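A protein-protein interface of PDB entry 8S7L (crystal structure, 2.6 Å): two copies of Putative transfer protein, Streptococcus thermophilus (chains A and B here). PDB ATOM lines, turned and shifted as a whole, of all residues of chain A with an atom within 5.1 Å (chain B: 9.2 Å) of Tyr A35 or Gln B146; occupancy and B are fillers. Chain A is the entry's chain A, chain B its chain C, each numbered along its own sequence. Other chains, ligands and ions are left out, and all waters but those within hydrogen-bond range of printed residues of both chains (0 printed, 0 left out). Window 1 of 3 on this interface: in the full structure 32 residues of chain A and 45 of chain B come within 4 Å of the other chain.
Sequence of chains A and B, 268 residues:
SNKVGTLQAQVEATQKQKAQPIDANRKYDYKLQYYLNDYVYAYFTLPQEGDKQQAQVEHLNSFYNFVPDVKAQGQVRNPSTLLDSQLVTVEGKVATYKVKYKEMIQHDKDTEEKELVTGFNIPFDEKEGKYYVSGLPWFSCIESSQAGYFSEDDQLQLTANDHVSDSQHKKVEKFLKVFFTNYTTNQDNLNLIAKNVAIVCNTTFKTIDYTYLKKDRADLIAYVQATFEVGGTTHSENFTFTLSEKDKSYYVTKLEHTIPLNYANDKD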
ATOM      1  N   TYR A  30       0.573  34.142 -10.845  1.00  0.00           N
ATOM      2  CA  TYR A  30       1.955  34.529 -10.568  1.00  0.00           C
ATOM      3  C   TYR A  30       2.908  33.321 -10.416  1.00  0.00           C
ATOM      4  O   TYR A  30       4.050  33.474 -10.001  1.00  0.00           O
ATOM      5  CB  TYR A  30       1.905  35.431  -9.337  1.00  0.00           C
ATOM      6  CG  TYR A  30       1.195  36.751  -9.584  1.00  0.00           C
ATOM      7  CD1 TYR A  30       1.769  37.770 -10.316  1.00  0.00           C
ATOM      8  CD2 TYR A  30      -0.037  37.002  -9.014  1.00  0.00           C
ATOM      9  CE1 TYR A  30       1.140  38.989 -10.492  1.00  0.00           C
ATOM     10  CE2 TYR A  30      -0.677  38.227  -9.174  1.00  0.00           C
ATOM     11  CZ  TYR A  30      -0.097  39.211  -9.930  1.00  0.00           C
ATOM     12  OH  TYR A  30      -0.735  40.396 -10.081  1.00  0.00           O
ATOM     13  N   LYS A  31       2.475  32.123 -10.783  1.00  0.00           N
ATOM     14  CA  LYS A  31       3.268  30.967 -10.362  1.00  0.00           C
ATOM     15  C   LYS A  31       4.659  31.002 -11.000  1.00  0.00           C
ATOM     16  O   LYS A  31       5.678  30.843 -10.287  1.00  0.00           O
ATOM     17  CB  LYS A  31       2.815  29.554 -10.776  1.00  0.00           C
ATOM     18  CG  LYS A  31       1.531  29.070 -10.108  1.00  0.00           C
ATOM     19  CD  LYS A  31       0.934  27.739 -10.553  1.00  0.00           C
ATOM     20  CE  LYS A  31      -0.235  27.482  -9.630  1.00  0.00           C
ATOM     21  NZ  LYS A  31      -1.171  26.431 -10.027  1.00  0.00           N
ATOM     22  N   LEU A  32       4.661  31.203 -12.347  1.00  0.00           N
ATOM     23  CA  LEU A  32       5.881  31.387 -13.128  1.00  0.00           C
ATOM     24  C   LEU A  32       6.772  32.503 -12.569  1.00  0.00           C
ATOM     25  O   LEU A  32       7.971  32.310 -12.310  1.00  0.00           O
ATOM     26  CB  LEU A  32       5.537  31.675 -14.564  1.00  0.00           C
ATOM     27  CG  LEU A  32       6.720  31.825 -15.516  1.00  0.00           C
ATOM     28  CD1 LEU A  32       7.603  30.606 -15.528  1.00  0.00           C
ATOM     29  CD2 LEU A  32       6.180  32.165 -16.872  1.00  0.00           C
ATOM     30  N   GLN A  33       6.148  33.678 -12.385  1.00  0.00           N
ATOM     31  CA  GLN A  33       6.891  34.820 -11.893  1.00  0.00           C
ATOM     32  C   GLN A  33       7.571  34.543 -10.552  1.00  0.00           C
ATOM     33  O   GLN A  33       8.699  34.959 -10.357  1.00  0.00           O
ATOM     34  CB  GLN A  33       5.969  36.035 -11.853  1.00  0.00           C
ATOM     35  CG  GLN A  33       6.598  37.168 -11.053  1.00  0.00           C
ATOM     36  CD  GLN A  33       5.948  38.513 -11.270  1.00  0.00           C
ATOM     37  OE1 GLN A  33       4.785  38.652 -11.632  1.00  0.00           O
ATOM     38  NE2 GLN A  33       6.716  39.546 -11.042  1.00  0.00           N
ATOM     39  N   TYR A  34       6.889  33.856  -9.629  1.00  0.00           N
ATOM     40  CA  TYR A  34       7.461  33.598  -8.313  1.00  0.00           C
ATOM     41  C   TYR A  34       8.596  32.589  -8.459  1.00  0.00           C
ATOM     42  O   TYR A  34       9.601  32.663  -7.740  1.00  0.00           O
ATOM     43  CB  TYR A  34       6.448  33.146  -7.258  1.00  0.00           C
ATOM     44  CG  TYR A  34       5.323  34.131  -6.934  1.00  0.00           C
ATOM     45  CD1 TYR A  34       5.498  35.509  -7.039  1.00  0.00           C
ATOM     46  CD2 TYR A  34       4.086  33.674  -6.541  1.00  0.00           C
ATOM     47  CE1 TYR A  34       4.478  36.396  -6.748  1.00  0.00           C
ATOM     48  CE2 TYR A  34       3.056  34.545  -6.204  1.00  0.00           C
ATOM     49  CZ  TYR A  34       3.269  35.908  -6.317  1.00  0.00           C
ATOM     50  OH  TYR A  34       2.304  36.799  -6.057  1.00  0.00           O
ATOM     51  N   TYR A  35       8.406  31.680  -9.424  1.00  0.00           N
ATOM     52  CA  TYR A  35       9.424  30.674  -9.699  1.00  0.00           C
ATOM     53  C   TYR A  35      10.705  31.392 -10.158  1.00  0.00           C
ATOM     54  O   TYR A  35      11.797  31.220  -9.595  1.00  0.00           O
ATOM     55  CB  TYR A  35       8.817  29.668 -10.692  1.00  0.00           C
ATOM     56  CG  TYR A  35       9.860  28.655 -11.141  1.00  0.00           C
ATOM     57  CD1 TYR A  35      10.279  27.654 -10.270  1.00  0.00           C
ATOM     58  CD2 TYR A  35      10.506  28.741 -12.379  1.00  0.00           C
ATOM     59  CE1 TYR A  35      11.307  26.778 -10.605  1.00  0.00           C
ATOM     60  CE2 TYR A  35      11.540  27.881 -12.705  1.00  0.00           C
ATOM     61  CZ  TYR A  35      11.931  26.885 -11.833  1.00  0.00           C
ATOM     62  OH  TYR A  35      12.918  26.000 -12.155  1.00  0.00           O
ATOM     63  N   LEU A  36      10.555  32.205 -11.208  1.00  0.00           N
ATOM     64  CA  LEU A  36      11.730  32.857 -11.773  1.00  0.00           C
ATOM     65  C   LEU A  36      12.333  33.816 -10.760  1.00  0.00           C
ATOM     66  O   LEU A  36      13.552  33.979 -10.691  1.00  0.00           O
ATOM     67  CB  LEU A  36      11.332  33.518 -13.095  1.00  0.00           C
ATOM     68  CG  LEU A  36      10.807  32.520 -14.142  1.00  0.00           C
ATOM     69  CD1 LEU A  36      10.278  33.147 -15.369  1.00  0.00           C
ATOM     70  CD2 LEU A  36      11.977  31.628 -14.492  1.00  0.00           C
ATOM     71  N   ASN A  37      11.501  34.348  -9.860  1.00  0.00           N
ATOM     72  CA  ASN A  37      12.059  35.209  -8.832  1.00  0.00           C
ATOM     73  C   ASN A  37      13.015  34.444  -7.952  1.00  0.00           C
ATOM     74  O   ASN A  37      14.052  34.978  -7.586  1.00  0.00           O
ATOM     75  CB  ASN A  37      11.004  35.805  -7.926  1.00  0.00           C
ATOM     76  CG  ASN A  37      10.232  36.883  -8.644  1.00  0.00           C
ATOM     77  OD1 ASN A  37      10.636  37.381  -9.708  1.00  0.00           O
ATOM     78  ND2 ASN A  37       9.096  37.216  -8.108  1.00  0.00           N
ATOM     79  N   ASP A  38      12.669  33.169  -7.700  1.00  0.00           N
ATOM     80  CA  ASP A  38      13.498  32.297  -6.867  1.00  0.00           C
ATOM     81  C   ASP A  38      14.784  31.982  -7.631  1.00  0.00           C
ATOM     82  O   ASP A  38      15.890  32.063  -7.096  1.00  0.00           O
ATOM     83  CB  ASP A  38      12.701  31.083  -6.347  1.00  0.00           C
ATOM     84  CG  ASP A  38      11.520  31.358  -5.404  1.00  0.00           C
ATOM     85  OD1 ASP A  38      11.457  32.494  -4.833  1.00  0.00           O
ATOM     86  OD2 ASP A  38      10.517  30.567  -5.425  1.00  0.00           O
ATOM     87  N   TYR A  39      14.649  31.654  -8.924  1.00  0.00           N
ATOM     88  CA  TYR A  39      15.839  31.414  -9.732  1.00  0.00           C
ATOM     89  C   TYR A  39      16.786  32.611  -9.619  1.00  0.00           C
ATOM     90  O   TYR A  39      17.951  32.473  -9.245  1.00  0.00           O
ATOM     91  CB  TYR A  39      15.478  31.118 -11.182  1.00  0.00           C
ATOM     92  CG  TYR A  39      16.720  30.948 -12.052  1.00  0.00           C
ATOM     93  CD1 TYR A  39      17.561  29.874 -11.855  1.00  0.00           C
ATOM     94  CD2 TYR A  39      17.011  31.813 -13.103  1.00  0.00           C
ATOM     95  CE1 TYR A  39      18.714  29.727 -12.594  1.00  0.00           C
ATOM     96  CE2 TYR A  39      18.141  31.659 -13.868  1.00  0.00           C
ATOM     97  CZ  TYR A  39      19.004  30.624 -13.596  1.00  0.00           C
ATOM     98  OH  TYR A  39      20.120  30.408 -14.324  1.00  0.00           O
ATOM     99  N   SER A  62      19.374  22.948  -8.884  1.00  0.00           N
ATOM    100  CA  SER A  62      18.068  22.305  -8.757  1.00  0.00           C
ATOM    101  C   SER A  62      17.010  22.939  -9.665  1.00  0.00           C
ATOM    102  O   SER A  62      15.962  22.341  -9.856  1.00  0.00           O
ATOM    103  CB  SER A  62      17.596  22.331  -7.335  1.00  0.00           C
ATOM    104  OG  SER A  62      16.846  23.513  -7.104  1.00  0.00           O
ATOM    105  N   PHE A  63      17.289  24.157 -10.190  1.00  0.00           N
ATOM    106  CA  PHE A  63      16.330  24.821 -11.053  1.00  0.00           C
ATOM    107  C   PHE A  63      16.362  24.238 -12.463  1.00  0.00           C
ATOM    108  O   PHE A  63      15.362  24.304 -13.180  1.00  0.00           O
ATOM    109  CB  PHE A  63      16.584  26.317 -11.067  1.00  0.00           C
ATOM    110  CG  PHE A  63      16.076  26.983  -9.808  1.00  0.00           C
ATOM    111  CD1 PHE A  63      14.755  27.413  -9.715  1.00  0.00           C
ATOM    112  CD2 PHE A  63      16.922  27.172  -8.726  1.00  0.00           C
ATOM    113  CE1 PHE A  63      14.275  28.040  -8.562  1.00  0.00           C
ATOM    114  CE2 PHE A  63      16.460  27.823  -7.570  1.00  0.00           C
ATOM    115  CZ  PHE A  63      15.148  28.252  -7.483  1.00  0.00           C
ATOM    116  N   TYR A  64      17.518  23.734 -12.897  1.00  0.00           N
ATOM    117  CA  TYR A  64      17.617  23.311 -14.270  1.00  0.00           C
ATOM    118  C   TYR A  64      17.047  21.911 -14.414  1.00  0.00           C
ATOM    119  O   TYR A  64      17.035  21.133 -13.478  1.00  0.00           O
ATOM    120  CB  TYR A  64      19.046  23.362 -14.804  1.00  0.00           C
ATOM    121  CG  TYR A  64      19.769  24.701 -14.655  1.00  0.00           C
ATOM    122  CD1 TYR A  64      19.646  25.689 -15.609  1.00  0.00           C
ATOM    123  CD2 TYR A  64      20.604  24.943 -13.603  1.00  0.00           C
ATOM    124  CE1 TYR A  64      20.325  26.894 -15.488  1.00  0.00           C
ATOM    125  CE2 TYR A  64      21.275  26.143 -13.454  1.00  0.00           C
ATOM    126  CZ  TYR A  64      21.125  27.119 -14.398  1.00  0.00           C
ATOM    127  OH  TYR A  64      21.797  28.283 -14.234  1.00  0.00           O
ATOM    128  N   LYS A 130       4.494  22.393 -14.358  1.00  0.00           N
ATOM    129  CA  LYS A 130       5.669  22.709 -13.568  1.00  0.00           C
ATOM    130  C   LYS A 130       6.720  23.417 -14.405  1.00  0.00           C
ATOM    131  O   LYS A 130       6.696  23.364 -15.632  1.00  0.00           O
ATOM    132  CB  LYS A 130       6.125  21.462 -12.827  1.00  0.00           C
ATOM    133  CG  LYS A 130       5.086  21.316 -11.748  1.00  0.00           C
ATOM    134  CD  LYS A 130       5.769  20.613 -10.578  1.00  0.00           C
ATOM    135  CE  LYS A 130       4.970  19.923  -9.475  1.00  0.00           C
ATOM    136  NZ  LYS A 130       4.029  20.869  -8.863  1.00  0.00           N
ATOM    137  N   TYR A 131       7.651  24.094 -13.738  1.00  0.00           N
ATOM    138  CA  TYR A 131       8.565  24.943 -14.490  1.00  0.00           C
ATOM    139  C   TYR A 131      10.001  24.479 -14.216  1.00  0.00           C
ATOM    140  O   TYR A 131      10.299  23.862 -13.187  1.00  0.00           O
ATOM    141  CB  TYR A 131       8.299  26.397 -14.056  1.00  0.00           C
ATOM    142  CG  TYR A 131       6.908  26.901 -14.423  1.00  0.00           C
ATOM    143  CD1 TYR A 131       6.539  26.982 -15.764  1.00  0.00           C
ATOM    144  CD2 TYR A 131       5.996  27.366 -13.469  1.00  0.00           C
ATOM    145  CE1 TYR A 131       5.300  27.493 -16.123  1.00  0.00           C
ATOM    146  CE2 TYR A 131       4.740  27.890 -13.808  1.00  0.00           C
ATOM    147  CZ  TYR A 131       4.398  27.954 -15.152  1.00  0.00           C
ATOM    148  OH  TYR A 131       3.241  28.399 -15.750  1.00  0.00           O
ATOM    149  N   TYR A 132      10.876  24.834 -15.168  1.00  0.00           N
ATOM    150  CA  TYR A 132      12.310  24.626 -15.073  1.00  0.00           C
ATOM    151  C   TYR A 132      13.046  25.613 -15.972  1.00  0.00           C
ATOM    152  O   TYR A 132      12.519  26.077 -16.977  1.00  0.00           O
ATOM    153  CB  TYR A 132      12.721  23.205 -15.482  1.00  0.00           C
ATOM    154  CG  TYR A 132      12.317  22.766 -16.887  1.00  0.00           C
ATOM    155  CD1 TYR A 132      11.053  22.279 -17.144  1.00  0.00           C
ATOM    156  CD2 TYR A 132      13.215  22.720 -17.931  1.00  0.00           C
ATOM    157  CE1 TYR A 132      10.695  21.823 -18.401  1.00  0.00           C
ATOM    158  CE2 TYR A 132      12.868  22.224 -19.189  1.00  0.00           C
ATOM    159  CZ  TYR A 132      11.597  21.775 -19.420  1.00  0.00           C
ATOM    160  OH  TYR A 132      11.127  21.365 -20.632  1.00  0.00           O
ATOM    161  N   VAL A 133      14.306  25.868 -15.602  1.00  0.00           N
ATOM    162  CA  VAL A 133      15.215  26.670 -16.376  1.00  0.00           C
ATOM    163  C   VAL A 133      15.922  25.675 -17.296  1.00  0.00           C
ATOM    164  O   VAL A 133      16.457  24.670 -16.817  1.00  0.00           O
ATOM    165  CB  VAL A 133      16.217  27.447 -15.514  1.00  0.00           C
ATOM    166  CG1 VAL A 133      17.329  28.073 -16.353  1.00  0.00           C
ATOM    167  CG2 VAL A 133      15.537  28.484 -14.594  1.00  0.00           C
ATOM    168  N   GLN B  86       1.629  36.283  -0.627  1.00  0.00           N
ATOM    169  CA  GLN B  86       1.623  36.443  -2.058  1.00  0.00           C
ATOM    170  C   GLN B  86       0.459  35.696  -2.682  1.00  0.00           C
ATOM    171  O   GLN B  86       0.334  34.472  -2.533  1.00  0.00           O
ATOM    172  CB  GLN B  86       2.930  35.868  -2.585  1.00  0.00           C
ATOM    173  CG  GLN B  86       4.120  36.756  -2.273  1.00  0.00           C
ATOM    174  CD  GLN B  86       5.407  36.046  -2.585  1.00  0.00           C
ATOM    175  OE1 GLN B  86       5.921  35.375  -1.700  1.00  0.00           O
ATOM    176  NE2 GLN B  86       5.896  36.121  -3.820  1.00  0.00           N
ATOM    177  N   VAL B  88      -1.141  33.839  -5.570  1.00  0.00           N
ATOM    178  CA  VAL B  88      -0.513  33.074  -6.629  1.00  0.00           C
ATOM    179  C   VAL B  88      -1.486  32.941  -7.785  1.00  0.00           C
ATOM    180  O   VAL B  88      -1.080  33.129  -8.945  1.00  0.00           O
ATOM    181  CB  VAL B  88       0.146  31.732  -6.232  1.00  0.00           C
ATOM    182  CG1 VAL B  88       0.084  31.395  -4.757  1.00  0.00           C
ATOM    183  CG2 VAL B  88      -0.316  30.594  -7.063  1.00  0.00           C
ATOM    184  N   LYS B  98      -0.087  32.074  -0.783  1.00  0.00           N
ATOM    185  CA  LYS B  98       0.982  31.370  -0.098  1.00  0.00           C
ATOM    186  C   LYS B  98       1.356  32.336   1.016  1.00  0.00           C
ATOM    187  O   LYS B  98       1.486  33.532   0.789  1.00  0.00           O
ATOM    188  CB  LYS B  98       2.036  30.842  -1.093  1.00  0.00           C
ATOM    189  CG  LYS B  98       3.405  31.467  -1.160  1.00  0.00           C
ATOM    190  CD  LYS B  98       4.058  31.748  -2.528  1.00  0.00           C
ATOM    191  CE  LYS B  98       5.179  30.864  -2.956  1.00  0.00           C
ATOM    192  NZ  LYS B  98       5.575  31.345  -4.264  1.00  0.00           N
ATOM    193  N   GLU B 143       2.032  24.503  -3.335  1.00  0.00           N
ATOM    194  CA  GLU B 143       2.570  23.817  -4.492  1.00  0.00           C
ATOM    195  C   GLU B 143       4.022  24.217  -4.712  1.00  0.00           C
ATOM    196  O   GLU B 143       4.389  25.396  -4.653  1.00  0.00           O
ATOM    197  CB  GLU B 143       1.838  24.164  -5.783  1.00  0.00           C
ATOM    198  CG  GLU B 143       0.377  23.730  -5.799  1.00  0.00           C
ATOM    199  CD  GLU B 143       0.009  23.479  -7.246  1.00  0.00           C
ATOM    200  OE1 GLU B 143       0.450  24.292  -8.148  1.00  0.00           O
ATOM    201  OE2 GLU B 143      -0.682  22.430  -7.426  1.00  0.00           O
ATOM    202  N   SER B 144       4.823  23.173  -4.894  1.00  0.00           N
ATOM    203  CA  SER B 144       6.152  23.252  -5.454  1.00  0.00           C
ATOM    204  C   SER B 144       6.036  23.614  -6.933  1.00  0.00           C
ATOM    205  O   SER B 144       5.266  23.009  -7.677  1.00  0.00           O
ATOM    206  CB  SER B 144       6.833  21.936  -5.321  1.00  0.00           C
ATOM    207  OG  SER B 144       8.029  21.983  -6.087  1.00  0.00           O
ATOM    208  N   SER B 145       6.834  24.568  -7.397  1.00  0.00           N
ATOM    209  CA  SER B 145       6.699  24.935  -8.788  1.00  0.00           C
ATOM    210  C   SER B 145       7.741  24.241  -9.665  1.00  0.00           C
ATOM    211  O   SER B 145       7.540  24.184 -10.866  1.00  0.00           O
ATOM    212  CB  SER B 145       6.699  26.392  -8.910  1.00  0.00           C
ATOM    213  OG  SER B 145       5.366  26.880  -8.810  1.00  0.00           O
ATOM    214  N   GLN B 146       8.739  23.559  -9.069  1.00  0.00           N
ATOM    215  CA  GLN B 146       9.862  23.027  -9.832  1.00  0.00           C
ATOM    216  C   GLN B 146       9.567  21.705 -10.544  1.00  0.00           C
ATOM    217  O   GLN B 146       9.189  20.743  -9.922  1.00  0.00           O
ATOM    218  CB  GLN B 146      10.983  22.802  -8.829  1.00  0.00           C
ATOM    219  CG  GLN B 146      12.200  22.134  -9.438  1.00  0.00           C
ATOM    220  CD  GLN B 146      12.935  23.090 -10.342  1.00  0.00           C
ATOM    221  OE1 GLN B 146      13.346  24.181  -9.913  1.00  0.00           O
ATOM    222  NE2 GLN B 146      13.118  22.655 -11.584  1.00  0.00           N
ATOM    223  N   ALA B 147       9.846  21.597 -11.837  1.00  0.00           N
ATOM    224  CA  ALA B 147       9.522  20.376 -12.568  1.00  0.00           C
ATOM    225  C   ALA B 147      10.627  19.376 -12.307  1.00  0.00           C
ATOM    226  O   ALA B 147      11.705  19.820 -11.942  1.00  0.00           O
ATOM    227  CB  ALA B 147       9.417  20.661 -14.052  1.00  0.00           C
ATOM    228  N   GLY B 148      10.359  18.074 -12.540  1.00  0.00           N
ATOM    229  CA  GLY B 148      11.416  17.057 -12.461  1.00  0.00           C
ATOM    230  C   GLY B 148      11.118  15.771 -13.250  1.00  0.00           C
ATOM    231  O   GLY B 148      10.202  15.708 -14.058  1.00  0.00           O
ATOM    232  N   TYR B 149      11.950  14.743 -13.040  1.00  0.00           N
ATOM    233  CA  TYR B 149      11.731  13.399 -13.579  1.00  0.00           C
ATOM    234  C   TYR B 149      11.932  13.450 -15.095  1.00  0.00           C
ATOM    235  O   TYR B 149      11.140  12.939 -15.877  1.00  0.00           O
ATOM    236  CB  TYR B 149      10.414  12.834 -13.004  1.00  0.00           C
ATOM    237  CG  TYR B 149      10.518  12.706 -11.484  1.00  0.00           C
ATOM    238  CD1 TYR B 149      10.903  11.510 -10.881  1.00  0.00           C
ATOM    239  CD2 TYR B 149      10.354  13.824 -10.661  1.00  0.00           C
ATOM    240  CE1 TYR B 149      11.061  11.420  -9.505  1.00  0.00           C
ATOM    241  CE2 TYR B 149      10.524  13.753  -9.287  1.00  0.00           C
ATOM    242  CZ  TYR B 149      10.870  12.544  -8.714  1.00  0.00           C
ATOM    243  OH  TYR B 149      11.022  12.487  -7.367  1.00  0.00           O
ATOM    244  N   PHE B 150      13.048  14.045 -15.517  1.00  0.00           N
ATOM    245  CA  PHE B 150      13.215  14.372 -16.913  1.00  0.00           C
ATOM    246  C   PHE B 150      13.840  13.213 -17.659  1.00  0.00           C
ATOM    247  O   PHE B 150      14.818  12.679 -17.160  1.00  0.00           O
ATOM    248  CB  PHE B 150      14.168  15.555 -17.063  1.00  0.00           C
ATOM    249  CG  PHE B 150      13.625  16.870 -16.515  1.00  0.00           C
ATOM    250  CD1 PHE B 150      12.637  17.578 -17.209  1.00  0.00           C
ATOM    251  CD2 PHE B 150      14.103  17.384 -15.313  1.00  0.00           C
ATOM    252  CE1 PHE B 150      12.153  18.775 -16.717  1.00  0.00           C
ATOM    253  CE2 PHE B 150      13.605  18.582 -14.816  1.00  0.00           C
ATOM    254  CZ  PHE B 150      12.640  19.281 -15.523  1.00  0.00           C
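N of Tyr A30 lies within hydrogen-bond range of O of Val B88 (2.7 Å).
NZ of Lys A31 is in salt-bridge range of OE1 of Glu B143, 3.3 Å away.
The side-chain amide oxygen (OE1) of Gln B146 sits at hydrogen-bond distance from the side-chain hydroxyl (OH) of Tyr A35 (2.9 Å).
The backbone carbonyl oxygen (O) of Ser A62 sits close to the side-chain amide oxygen (OE1) of Gln B146, at 3.2 Å.
The side-chain amide nitrogen (NE2) of Gln B146 is in hydrogen-bond range of the backbone carbonyl oxygen (O) of Phe A63 (3.2 Å).
NZ of Lys A130 is in hydrogen-bond range of O of Ser B144 (2.7 Å).
O of Ser B145 lies within hydrogen-bond range of N of Tyr A131 (2.9 Å).
The side-chain amide nitrogen of Gln B146 lies within hydrogen-bond range of the backbone carbonyl oxygen of Tyr A131.
O of Tyr A131 sits at hydrogen-bond distance from N of Ala B147 (2.7 Å).
Val B88 touches Lys A31 (CG2 to CG, 3.9 Å).
Gln B86 touches Tyr A34.
Val B88 touches Tyr A34.
Tyr A34 touches Lys B98.
O of Ser B145 touches CA of Lys A130, at 3.6 Å.
Lys A130 touches Gln B146 (CD to O, 3.5 Å).
CB of Lys A130 touches CA of Ala B147, at 3.6 Å.
Tyr A132 touches Gln B146.
Ala B147 touches Tyr A132 (CB to CD1, 3.9 Å).
CE1 of Phe B150 touches CD1 of Tyr A132 (3.7 Å).
Hydrophobic or aromatic side chains of chain B within 4 Å of the printed part of chain A: Val B88, Ala B147 and Phe B150.
Of the 17 printed residues of chain A, 9 touch a printed residue of chain B.
Among the printed residues, Asp or Glu carboxylates within 4 Å of a Lys or Arg side-chain nitrogen of the other chain: Lys A31 with Glu B143 (3.3 Å).
No position is printed for both chains.
Of the 19 pairs that touch across the chains among the printed residues, none has its exchanged pair printed and touching as well.
The side-chain hydroxyl (OH) of Tyr A35 is in hydrogen-bond range of the backbone carbonyl oxygen (O) of Phe A63 (3.1 Å).
O of Phe A63 lies within hydrogen-bond range of N of Val A133, 3.1 Å away.
The backbone carbonyl oxygen (O) of Gln B86 is in hydrogen-bond range of the backbone NH (N) of Lys B98 (3.0 Å).
The side-chain hydroxyl (OG) of Ser B144 sits close to the backbone NH (N) of Gln B146 (3.4 Å).
Gln A33 touches none of the printed residues of chain B.
Of the printed residues of chain B, Tyr A34 touches Gln B86, Val B88 and Lys B98.
No residue of chain B comes within 4 Å of Asp A38.
Printed residues of chain B within 4 Å of Tyr A132: Gln B146, Ala B147 and Phe B150.
Printed residues of chain A within 4 Å of Val B88: Tyr A30, Lys A31 and Tyr A34.
Of the printed residues of chain A, Glu B143 touches Lys A31.
Gln B146 touches just these residues of chain A: Tyr A35, Ser A62, Phe A63, Lys A130, Tyr A131 and Tyr A132.
Of the printed residues of chain A, Ala B147 touches Lys A130, Tyr A131 and Tyr A132.
Gly B148 touches none of the printed residues of chain A.
The nearest residue of chain B that does not touch Tyr A35 is Ser B145 (4.03 Å).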
